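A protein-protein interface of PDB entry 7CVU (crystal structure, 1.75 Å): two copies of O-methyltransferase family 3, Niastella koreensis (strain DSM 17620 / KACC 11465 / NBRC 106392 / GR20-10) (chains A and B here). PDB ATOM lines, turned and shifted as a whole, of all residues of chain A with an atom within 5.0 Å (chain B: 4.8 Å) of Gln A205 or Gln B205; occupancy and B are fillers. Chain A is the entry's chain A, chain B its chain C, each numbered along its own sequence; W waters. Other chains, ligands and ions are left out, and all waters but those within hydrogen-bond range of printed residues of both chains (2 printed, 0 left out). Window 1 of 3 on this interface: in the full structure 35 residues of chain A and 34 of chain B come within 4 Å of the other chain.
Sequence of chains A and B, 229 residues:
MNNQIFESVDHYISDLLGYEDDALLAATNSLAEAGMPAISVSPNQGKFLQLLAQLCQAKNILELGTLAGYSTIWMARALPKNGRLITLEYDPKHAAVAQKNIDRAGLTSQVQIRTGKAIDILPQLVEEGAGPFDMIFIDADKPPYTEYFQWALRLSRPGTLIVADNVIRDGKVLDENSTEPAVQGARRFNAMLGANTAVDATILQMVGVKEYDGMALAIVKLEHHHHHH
Hydrophobic or aromatic side chains of chain B that line the printed part of chain A: Phe B6, Val B9, Ile B13, Ile B168, Ile B203, Met B206, Val B207 and Tyr B212.
The side-chain hydroxyl (OH) of Tyr A212 sits at hydrogen-bond distance from the side-chain amide oxygen (OE1) of Gln A205, at 2.6 Å.
OE1 of Gln B205 is in hydrogen-bond range of OH of Tyr B212.
N of Met A206 is in hydrogen-bond range of O of Asp A213 (2.6 Å).
N of Asp B213 sits at hydrogen-bond distance from O of Met B206.
Water W1 bridges OD1 of Asp B10 (2.8 Å) and NE2 of Gln A205 (2.8 Å).
Water W2 lies within hydrogen-bond range of N of Gln A205 (2.9 Å) and O of Val B207 (3.0 Å).
The side-chain amide nitrogen (NE2) of Gln B205 sits at hydrogen-bond distance from the side-chain carboxylate (OD1) of Asp A10 (3.3 Å).
O of Gln A205 sits at hydrogen-bond distance from N of Val B207.
N of Asp B10 lies close to NE2 of Gln A205 (3.4 Å).
The side-chain amide nitrogen (NE2) of Gln A205 sits at hydrogen-bond distance from the backbone carbonyl oxygen (O) of Phe B6.
O of Phe A6 is in hydrogen-bond range of NE2 of Gln B205.
The backbone carbonyl oxygen (O) of Gln B205 is in hydrogen-bond range of the backbone NH (N) of Val A207 (3.2 Å).
Val A9 touches Tyr B212, and with the chains exchanged Tyr A212 touches Val B9.
Ile A13 touches Ile B203, and with the chains exchanged Ile A203 touches Ile B13.
Ile A13 touches Gln B205, and with the chains exchanged Gln A205 touches Ile B13.
Val A207 touches its own counterpart, Val B207.
Positions printed for both chains: 6, 9, 10, 13, 203, 204, 205, 206, 207, 208, 212, 213 and 214.
Of the 27 pairs that touch across the chains among the printed residues, 23 have their exchanged pair printed and touching as well.
Among the printed residues, pairs that only touch across the chains: Ile A5 with Tyr B212 (3.8 Å), Phe A6 with Phe B6 (3.7 Å), Phe A6 with Val B207 (3.7 Å), Phe A6 with Tyr B212 (3.7 Å), Val A9 with Ile B168 (3.8 Å), Val A9 with Gln B205 (3.5 Å), Val A9 with Tyr B212 (3.5 Å), Ile A13 with Ile B203 (3.6 Å), Ile A13 with Gln B205 (3.9 Å), Ile A203 with Ile B13 (3.6 Å), Gln A205 with Val B9 (3.4 Å), Gln A205 with Ile B13 (3.9 Å), Gln A205 with Gln B205 (3.98 Å), Gln A205 with Met B206 (3.2 Å), Gln A205 with Gly B208 (3.6 Å), Met A206 with Gln B205 (3.6 Å), Val A207 with Val B207 (3.9 Å), Gly A208 with Gln B205 (3.7 Å), Tyr A212 with Phe B6 (3.4 Å), Tyr A212 with Val B9 (3.5 Å) and Tyr A212 with Val B207 (3.9 Å).
Of the printed residues of chain B, Asp A10 touches Gln B205.
Printed residues of chain B within 4 Å of Ile A13: Ile B203 (3.6 Å) and Gln B205 (3.9 Å).
Printed residues of chain B within 4 Å of Gln A205: Phe B6 (3.2 Å), Val B9 (3.4 Å), Asp B10 (3.4 Å), Ile B13 (3.9 Å), Gln B205 (3.98 Å), Met B206 (3.2 Å), Val B207 (3.1 Å) and Gly B208 (3.6 Å).
Printed residues of chain B within 4 Å of Tyr A212: Phe B6 (3.4 Å), Val B9 (3.5 Å) and Val B207 (3.9 Å).
Asp A213 touches none of the printed residues of chain B.
Printed residues of chain A within 4 Å of Gln B205: Phe A6, Val A9, Asp A10, Ile A13, Gln A205, Met A206, Val A207 and Gly A208.
The nearest printed residue of chain B that does not touch Gln A205 is Asp B213 (7.0 Å).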
ATOM      1  N   ILE A   5     -34.189 -21.232 -28.725  1.00  0.00           N
ATOM      2  CA  ILE A   5     -33.877 -21.083 -27.285  1.00  0.00           C
ATOM      3  C   ILE A   5     -32.410 -20.665 -27.105  1.00  0.00           C
ATOM      4  O   ILE A   5     -32.142 -19.837 -26.204  1.00  0.00           O
ATOM      5  CB  ILE A   5     -34.234 -22.341 -26.473  1.00  0.00           C
ATOM      6  CG1 ILE A   5     -34.260 -21.991 -24.999  1.00  0.00           C
ATOM      7  CG2 ILE A   5     -33.343 -23.515 -26.791  1.00  0.00           C
ATOM      8  CD1 ILE A   5     -35.167 -20.862 -24.681  1.00  0.00           C
ATOM      9  N   PHE A   6     -31.475 -21.148 -27.940  1.00  0.00           N
ATOM     10  CA  PHE A   6     -30.046 -20.749 -27.796  1.00  0.00           C
ATOM     11  C   PHE A   6     -29.882 -19.269 -28.145  1.00  0.00           C
ATOM     12  O   PHE A   6     -29.152 -18.557 -27.455  1.00  0.00           O
ATOM     13  CB  PHE A   6     -29.114 -21.556 -28.688  1.00  0.00           C
ATOM     14  CG  PHE A   6     -29.260 -23.052 -28.611  1.00  0.00           C
ATOM     15  CD1 PHE A   6     -29.641 -23.677 -27.438  1.00  0.00           C
ATOM     16  CD2 PHE A   6     -28.935 -23.848 -29.710  1.00  0.00           C
ATOM     17  CE1 PHE A   6     -29.784 -25.052 -27.385  1.00  0.00           C
ATOM     18  CE2 PHE A   6     -29.073 -25.227 -29.651  1.00  0.00           C
ATOM     19  CZ  PHE A   6     -29.470 -25.833 -28.482  1.00  0.00           C
ATOM     20  N   VAL A   9     -31.664 -17.064 -25.182  1.00  0.00           N
ATOM     21  CA  VAL A   9     -30.819 -17.144 -23.954  1.00  0.00           C
ATOM     22  C   VAL A   9     -29.555 -16.332 -24.215  1.00  0.00           C
ATOM     23  O   VAL A   9     -29.117 -15.668 -23.299  1.00  0.00           O
ATOM     24  CB  VAL A   9     -30.531 -18.587 -23.487  1.00  0.00           C
ATOM     25  CG1 VAL A   9     -29.515 -18.661 -22.356  1.00  0.00           C
ATOM     26  CG2 VAL A   9     -31.813 -19.245 -23.031  1.00  0.00           C
ATOM     27  N   ASP A  10     -29.002 -16.362 -25.433  1.00  0.00           N
ATOM     28  CA  ASP A  10     -27.732 -15.616 -25.685  1.00  0.00           C
ATOM     29  C   ASP A  10     -27.991 -14.112 -25.602  1.00  0.00           C
ATOM     30  O   ASP A  10     -27.185 -13.399 -25.006  1.00  0.00           O
ATOM     31  CB  ASP A  10     -27.096 -15.954 -27.011  1.00  0.00           C
ATOM     32  CG  ASP A  10     -25.582 -16.158 -26.846  1.00  0.00           C
ATOM     33  OD1 ASP A  10     -25.134 -16.628 -25.732  1.00  0.00           O
ATOM     34  OD2 ASP A  10     -24.886 -15.902 -27.775  1.00  0.00           O
ATOM     35  N   ILE A  13     -28.151 -13.243 -21.994  1.00  0.00           N
ATOM     36  CA  ILE A  13     -26.769 -13.245 -21.436  1.00  0.00           C
ATOM     37  C   ILE A  13     -26.063 -11.970 -21.889  1.00  0.00           C
ATOM     38  O   ILE A  13     -25.422 -11.321 -21.021  1.00  0.00           O
ATOM     39  CB  ILE A  13     -26.010 -14.536 -21.802  1.00  0.00           C
ATOM     40  CG1 ILE A  13     -26.621 -15.765 -21.119  1.00  0.00           C
ATOM     41  CG2 ILE A  13     -24.540 -14.367 -21.418  1.00  0.00           C
ATOM     42  CD1 ILE A  13     -26.050 -17.079 -21.611  1.00  0.00           C
ATOM     43  N   ILE A 203     -13.089 -30.247 -26.144  1.00  0.00           N
ATOM     44  CA  ILE A 203     -13.880 -29.503 -27.181  1.00  0.00           C
ATOM     45  C   ILE A 203     -15.212 -29.142 -26.518  1.00  0.00           C
ATOM     46  O   ILE A 203     -15.896 -30.059 -26.006  1.00  0.00           O
ATOM     47  CB  ILE A 203     -14.092 -30.322 -28.469  1.00  0.00           C
ATOM     48  CG1 ILE A 203     -12.754 -30.738 -29.097  1.00  0.00           C
ATOM     49  CG2 ILE A 203     -14.973 -29.570 -29.469  1.00  0.00           C
ATOM     50  CD1 ILE A 203     -12.890 -31.788 -30.165  1.00  0.00           C
ATOM     51  N   LEU A 204     -15.551 -27.842 -26.509  1.00  0.00           N
ATOM     52  CA  LEU A 204     -16.866 -27.338 -26.040  1.00  0.00           C
ATOM     53  C   LEU A 204     -17.844 -27.270 -27.210  1.00  0.00           C
ATOM     54  O   LEU A 204     -17.457 -26.779 -28.301  1.00  0.00           O
ATOM     55  CB  LEU A 204     -16.690 -25.948 -25.443  1.00  0.00           C
ATOM     56  CG  LEU A 204     -15.692 -25.867 -24.298  1.00  0.00           C
ATOM     57  CD1 LEU A 204     -15.573 -24.410 -23.859  1.00  0.00           C
ATOM     58  CD2 LEU A 204     -16.136 -26.728 -23.129  1.00  0.00           C
ATOM     59  N   GLN A 205     -19.076 -27.708 -26.979  1.00  0.00           N
ATOM     60  CA  GLN A 205     -20.190 -27.484 -27.942  1.00  0.00           C
ATOM     61  C   GLN A 205     -20.909 -26.183 -27.594  1.00  0.00           C
ATOM     62  O   GLN A 205     -21.686 -26.153 -26.627  1.00  0.00           O
ATOM     63  CB  GLN A 205     -21.184 -28.628 -27.862  1.00  0.00           C
ATOM     64  CG  GLN A 205     -20.580 -29.960 -28.300  1.00  0.00           C
ATOM     65  CD  GLN A 205     -21.650 -31.013 -28.462  1.00  0.00           C
ATOM     66  OE1 GLN A 205     -22.498 -30.915 -29.351  1.00  0.00           O
ATOM     67  NE2 GLN A 205     -21.679 -31.985 -27.563  1.00  0.00           N
ATOM     68  N   MET A 206     -20.607 -25.124 -28.303  1.00  0.00           N
ATOM     69  CA  MET A 206     -21.096 -23.791 -27.891  1.00  0.00           C
ATOM     70  C   MET A 206     -22.283 -23.373 -28.762  1.00  0.00           C
ATOM     71  O   MET A 206     -22.234 -23.487 -29.994  1.00  0.00           O
ATOM     72  CB  MET A 206     -19.940 -22.788 -27.949  1.00  0.00           C
ATOM     73  CG  MET A 206     -18.882 -23.120 -26.890  1.00  0.00           C
ATOM     74  SD  MET A 206     -17.495 -22.058 -26.998  1.00  0.00           S
ATOM     75  CE  MET A 206     -18.207 -20.428 -27.192  1.00  0.00           C
ATOM     76  N   VAL A 207     -23.297 -22.812 -28.121  1.00  0.00           N
ATOM     77  CA  VAL A 207     -24.495 -22.371 -28.850  1.00  0.00           C
ATOM     78  C   VAL A 207     -24.785 -20.940 -28.417  1.00  0.00           C
ATOM     79  O   VAL A 207     -24.259 -20.489 -27.390  1.00  0.00           O
ATOM     80  CB  VAL A 207     -25.696 -23.297 -28.600  1.00  0.00           C
ATOM     81  CG1 VAL A 207     -25.410 -24.721 -29.128  1.00  0.00           C
ATOM     82  CG2 VAL A 207     -26.094 -23.330 -27.138  1.00  0.00           C
ATOM     83  N   GLY A 208     -25.603 -20.271 -29.201  1.00  0.00           N
ATOM     84  CA  GLY A 208     -25.986 -18.870 -28.938  1.00  0.00           C
ATOM     85  C   GLY A 208     -26.331 -18.174 -30.226  1.00  0.00           C
ATOM     86  O   GLY A 208     -26.930 -18.815 -31.086  1.00  0.00           O
ATOM     87  N   TYR A 212     -24.231 -23.084 -34.157  1.00  0.00           N
ATOM     88  CA  TYR A 212     -23.644 -24.166 -33.328  1.00  0.00           C
ATOM     89  C   TYR A 212     -22.187 -24.401 -33.718  1.00  0.00           C
ATOM     90  O   TYR A 212     -21.888 -24.594 -34.924  1.00  0.00           O
ATOM     91  CB  TYR A 212     -24.499 -25.411 -33.531  1.00  0.00           C
ATOM     92  CG  TYR A 212     -23.900 -26.721 -33.093  1.00  0.00           C
ATOM     93  CD1 TYR A 212     -23.855 -27.077 -31.761  1.00  0.00           C
ATOM     94  CD2 TYR A 212     -23.453 -27.642 -34.018  1.00  0.00           C
ATOM     95  CE1 TYR A 212     -23.313 -28.292 -31.350  1.00  0.00           C
ATOM     96  CE2 TYR A 212     -22.922 -28.858 -33.635  1.00  0.00           C
ATOM     97  CZ  TYR A 212     -22.840 -29.186 -32.291  1.00  0.00           C
ATOM     98  OH  TYR A 212     -22.352 -30.401 -31.887  1.00  0.00           O
ATOM     99  N   ASP A 213     -21.313 -24.423 -32.723  1.00  0.00           N
ATOM    100  CA  ASP A 213     -19.851 -24.359 -32.883  1.00  0.00           C
ATOM    101  C   ASP A 213     -19.222 -25.362 -31.928  1.00  0.00           C
ATOM    102  O   ASP A 213     -19.697 -25.469 -30.765  1.00  0.00           O
ATOM    103  CB  ASP A 213     -19.394 -22.938 -32.543  1.00  0.00           C
ATOM    104  CG  ASP A 213     -17.902 -22.699 -32.719  1.00  0.00           C
ATOM    105  OD1 ASP A 213     -17.364 -22.980 -33.827  1.00  0.00           O
ATOM    106  OD2 ASP A 213     -17.312 -22.199 -31.770  1.00  0.00           O
ATOM    107  N   GLY A 214     -18.195 -26.074 -32.372  1.00  0.00           N
ATOM    108  CA  GLY A 214     -17.233 -26.708 -31.465  1.00  0.00           C
ATOM    109  C   GLY A 214     -15.959 -25.881 -31.307  1.00  0.00           C
ATOM    110  O   GLY A 214     -15.328 -25.519 -32.320  1.00  0.00           O
ATOM    111  N   PHE B   6     -26.448 -33.530 -30.415  1.00  0.00           N
ATOM    112  CA  PHE B   6     -25.568 -33.005 -29.328  1.00  0.00           C
ATOM    113  C   PHE B   6     -25.075 -34.167 -28.478  1.00  0.00           C
ATOM    114  O   PHE B   6     -23.922 -34.190 -28.076  1.00  0.00           O
ATOM    115  CB  PHE B   6     -26.298 -31.921 -28.529  1.00  0.00           C
ATOM    116  CG  PHE B   6     -26.777 -30.773 -29.390  1.00  0.00           C
ATOM    117  CD1 PHE B   6     -26.067 -30.363 -30.498  1.00  0.00           C
ATOM    118  CD2 PHE B   6     -27.972 -30.136 -29.102  1.00  0.00           C
ATOM    119  CE1 PHE B   6     -26.514 -29.322 -31.287  1.00  0.00           C
ATOM    120  CE2 PHE B   6     -28.419 -29.090 -29.888  1.00  0.00           C
ATOM    121  CZ  PHE B   6     -27.681 -28.680 -30.963  1.00  0.00           C
ATOM    122  N   VAL B   9     -22.329 -36.087 -30.534  1.00  0.00           N
ATOM    123  CA  VAL B   9     -21.086 -35.274 -30.552  1.00  0.00           C
ATOM    124  C   VAL B   9     -20.479 -35.312 -29.159  1.00  0.00           C
ATOM    125  O   VAL B   9     -19.234 -35.409 -29.050  1.00  0.00           O
ATOM    126  CB  VAL B   9     -21.366 -33.852 -31.056  1.00  0.00           C
ATOM    127  CG1 VAL B   9     -20.165 -32.970 -30.868  1.00  0.00           C
ATOM    128  CG2 VAL B   9     -21.778 -33.853 -32.537  1.00  0.00           C
ATOM    129  N   ASP B  10     -21.286 -35.315 -28.096  1.00  0.00           N
ATOM    130  CA  ASP B  10     -20.707 -35.356 -26.733  1.00  0.00           C
ATOM    131  C   ASP B  10     -19.928 -36.675 -26.524  1.00  0.00           C
ATOM    132  O   ASP B  10     -18.792 -36.712 -25.981  1.00  0.00           O
ATOM    133  CB  ASP B  10     -21.816 -35.248 -25.704  1.00  0.00           C
ATOM    134  CG  ASP B  10     -21.346 -35.361 -24.285  1.00  0.00           C
ATOM    135  OD1 ASP B  10     -20.805 -34.379 -23.776  1.00  0.00           O
ATOM    136  OD2 ASP B  10     -21.528 -36.442 -23.720  1.00  0.00           O
ATOM    137  N   ILE B  13     -16.619 -36.584 -28.468  1.00  0.00           N
ATOM    138  CA  ILE B  13     -15.649 -35.744 -27.714  1.00  0.00           C
ATOM    139  C   ILE B  13     -15.106 -36.509 -26.507  1.00  0.00           C
ATOM    140  O   ILE B  13     -13.886 -36.432 -26.280  1.00  0.00           O
ATOM    141  CB  ILE B  13     -16.289 -34.402 -27.304  1.00  0.00           C
ATOM    142  CG1 ILE B  13     -16.669 -33.590 -28.547  1.00  0.00           C
ATOM    143  CG2 ILE B  13     -15.307 -33.699 -26.389  1.00  0.00           C
ATOM    144  CD1 ILE B  13     -17.435 -32.331 -28.261  1.00  0.00           C
ATOM    145  N   ILE B 168     -29.051 -21.366 -16.316  1.00  0.00           N
ATOM    146  CA  ILE B 168     -30.053 -20.953 -17.355  1.00  0.00           C
ATOM    147  C   ILE B 168     -31.302 -21.850 -17.276  1.00  0.00           C
ATOM    148  O   ILE B 168     -32.323 -21.455 -17.887  1.00  0.00           O
ATOM    149  CB  ILE B 168     -29.471 -20.885 -18.777  1.00  0.00           C
ATOM    150  CG1 ILE B 168     -29.050 -22.268 -19.257  1.00  0.00           C
ATOM    151  CG2 ILE B 168     -28.346 -19.844 -18.892  1.00  0.00           C
ATOM    152  CD1 ILE B 168     -28.653 -22.315 -20.756  1.00  0.00           C
ATOM    153  N   ILE B 203     -21.664 -15.987 -19.148  1.00  0.00           N
ATOM    154  CA  ILE B 203     -22.378 -17.283 -18.994  1.00  0.00           C
ATOM    155  C   ILE B 203     -22.173 -18.024 -20.300  1.00  0.00           C
ATOM    156  O   ILE B 203     -22.507 -17.473 -21.379  1.00  0.00           O
ATOM    157  CB  ILE B 203     -23.854 -17.104 -18.597  1.00  0.00           C
ATOM    158  CG1 ILE B 203     -23.977 -16.329 -17.277  1.00  0.00           C
ATOM    159  CG2 ILE B 203     -24.532 -18.472 -18.504  1.00  0.00           C
ATOM    160  CD1 ILE B 203     -25.337 -15.781 -17.003  1.00  0.00           C
ATOM    161  N   LEU B 204     -21.589 -19.221 -20.204  1.00  0.00           N
ATOM    162  CA  LEU B 204     -21.275 -20.074 -21.359  1.00  0.00           C
ATOM    163  C   LEU B 204     -22.488 -20.947 -21.608  1.00  0.00           C
ATOM    164  O   LEU B 204     -22.834 -21.678 -20.669  1.00  0.00           O
ATOM    165  CB  LEU B 204     -20.140 -21.019 -21.001  1.00  0.00           C
ATOM    166  CG  LEU B 204     -18.767 -20.465 -20.730  1.00  0.00           C
ATOM    167  CD1 LEU B 204     -17.790 -21.636 -20.660  1.00  0.00           C
ATOM    168  CD2 LEU B 204     -18.336 -19.506 -21.807  1.00  0.00           C
ATOM    169  N   GLN B 205     -23.090 -20.889 -22.804  1.00  0.00           N
ATOM    170  CA  GLN B 205     -24.163 -21.846 -23.134  1.00  0.00           C
ATOM    171  C   GLN B 205     -23.523 -22.996 -23.874  1.00  0.00           C
ATOM    172  O   GLN B 205     -22.920 -22.749 -24.970  1.00  0.00           O
ATOM    173  CB  GLN B 205     -25.192 -21.335 -24.122  1.00  0.00           C
ATOM    174  CG  GLN B 205     -26.271 -20.462 -23.574  1.00  0.00           C
ATOM    175  CD  GLN B 205     -27.342 -20.263 -24.630  1.00  0.00           C
ATOM    176  OE1 GLN B 205     -28.308 -21.009 -24.719  1.00  0.00           O
ATOM    177  NE2 GLN B 205     -27.167 -19.245 -25.458  1.00  0.00           N
ATOM    178  N   MET B 206     -23.752 -24.171 -23.346  1.00  0.00           N
ATOM    179  CA  MET B 206     -23.175 -25.418 -23.861  1.00  0.00           C
ATOM    180  C   MET B 206     -24.287 -26.448 -24.089  1.00  0.00           C
ATOM    181  O   MET B 206     -25.271 -26.501 -23.299  1.00  0.00           O
ATOM    182  CB  MET B 206     -22.198 -25.981 -22.825  1.00  0.00           C
ATOM    183  CG  MET B 206     -20.919 -25.149 -22.680  1.00  0.00           C
ATOM    184  SD  MET B 206     -20.184 -25.361 -21.012  1.00  0.00           S
ATOM    185  CE  MET B 206     -19.820 -27.108 -21.083  1.00  0.00           C
ATOM    186  N   VAL B 207     -24.022 -27.361 -25.004  1.00  0.00           N
ATOM    187  CA  VAL B 207     -24.901 -28.550 -25.188  1.00  0.00           C
ATOM    188  C   VAL B 207     -24.011 -29.782 -25.093  1.00  0.00           C
ATOM    189  O   VAL B 207     -22.787 -29.624 -24.953  1.00  0.00           O
ATOM    190  CB  VAL B 207     -25.708 -28.463 -26.494  1.00  0.00           C
ATOM    191  CG1 VAL B 207     -26.749 -27.363 -26.443  1.00  0.00           C
ATOM    192  CG2 VAL B 207     -24.811 -28.331 -27.729  1.00  0.00           C
ATOM    193  N   GLY B 208     -24.647 -30.957 -25.025  1.00  0.00           N
ATOM    194  CA  GLY B 208     -23.945 -32.218 -24.797  1.00  0.00           C
ATOM    195  C   GLY B 208     -23.693 -32.358 -23.306  1.00  0.00           C
ATOM    196  O   GLY B 208     -24.283 -33.239 -22.669  1.00  0.00           O
ATOM    197  N   TYR B 212     -27.988 -29.616 -21.965  1.00  0.00           N
ATOM    198  CA  TYR B 212     -28.105 -28.139 -22.215  1.00  0.00           C
ATOM    199  C   TYR B 212     -27.811 -27.438 -20.894  1.00  0.00           C
ATOM    200  O   TYR B 212     -28.494 -27.713 -19.876  1.00  0.00           O
ATOM    201  CB  TYR B 212     -29.506 -27.781 -22.724  1.00  0.00           C
ATOM    202  CG  TYR B 212     -29.743 -26.324 -23.022  1.00  0.00           C
ATOM    203  CD1 TYR B 212     -28.759 -25.515 -23.570  1.00  0.00           C
ATOM    204  CD2 TYR B 212     -31.000 -25.776 -22.851  1.00  0.00           C
ATOM    205  CE1 TYR B 212     -28.989 -24.181 -23.837  1.00  0.00           C
ATOM    206  CE2 TYR B 212     -31.254 -24.462 -23.152  1.00  0.00           C
ATOM    207  CZ  TYR B 212     -30.244 -23.658 -23.643  1.00  0.00           C
ATOM    208  OH  TYR B 212     -30.475 -22.364 -23.980  1.00  0.00           O
ATOM    209  N   ASP B 213     -26.718 -26.686 -20.845  1.00  0.00           N
ATOM    210  CA  ASP B 213     -26.223 -26.130 -19.562  1.00  0.00           C
ATOM    211  C   ASP B 213     -25.816 -24.684 -19.775  1.00  0.00           C
ATOM    212  O   ASP B 213     -25.282 -24.355 -20.858  1.00  0.00           O
ATOM    213  CB  ASP B 213     -25.061 -26.945 -19.007  1.00  0.00           C
ATOM    214  CG  ASP B 213     -24.671 -26.603 -17.576  1.00  0.00           C
ATOM    215  OD1 ASP B 213     -25.468 -26.000 -16.870  1.00  0.00           O
ATOM    216  OD2 ASP B 213     -23.594 -27.055 -17.147  1.00  0.00           O
ATOM    217  N   GLY B 214     -26.027 -23.861 -18.748  1.00  0.00           N
ATOM    218  CA  GLY B 214     -25.387 -22.541 -18.666  1.00  0.00           C
ATOM    219  C   GLY B 214     -24.393 -22.512 -17.530  1.00  0.00           C
ATOM    220  O   GLY B 214     -24.784 -22.824 -16.374  1.00  0.00           O
HETATM  221  O   HOH W   1     -20.100 -32.077 -25.199  1.00  0.00           O
HETATM  222  O   HOH W   2     -19.946 -28.659 -24.437  1.00  0.00           O
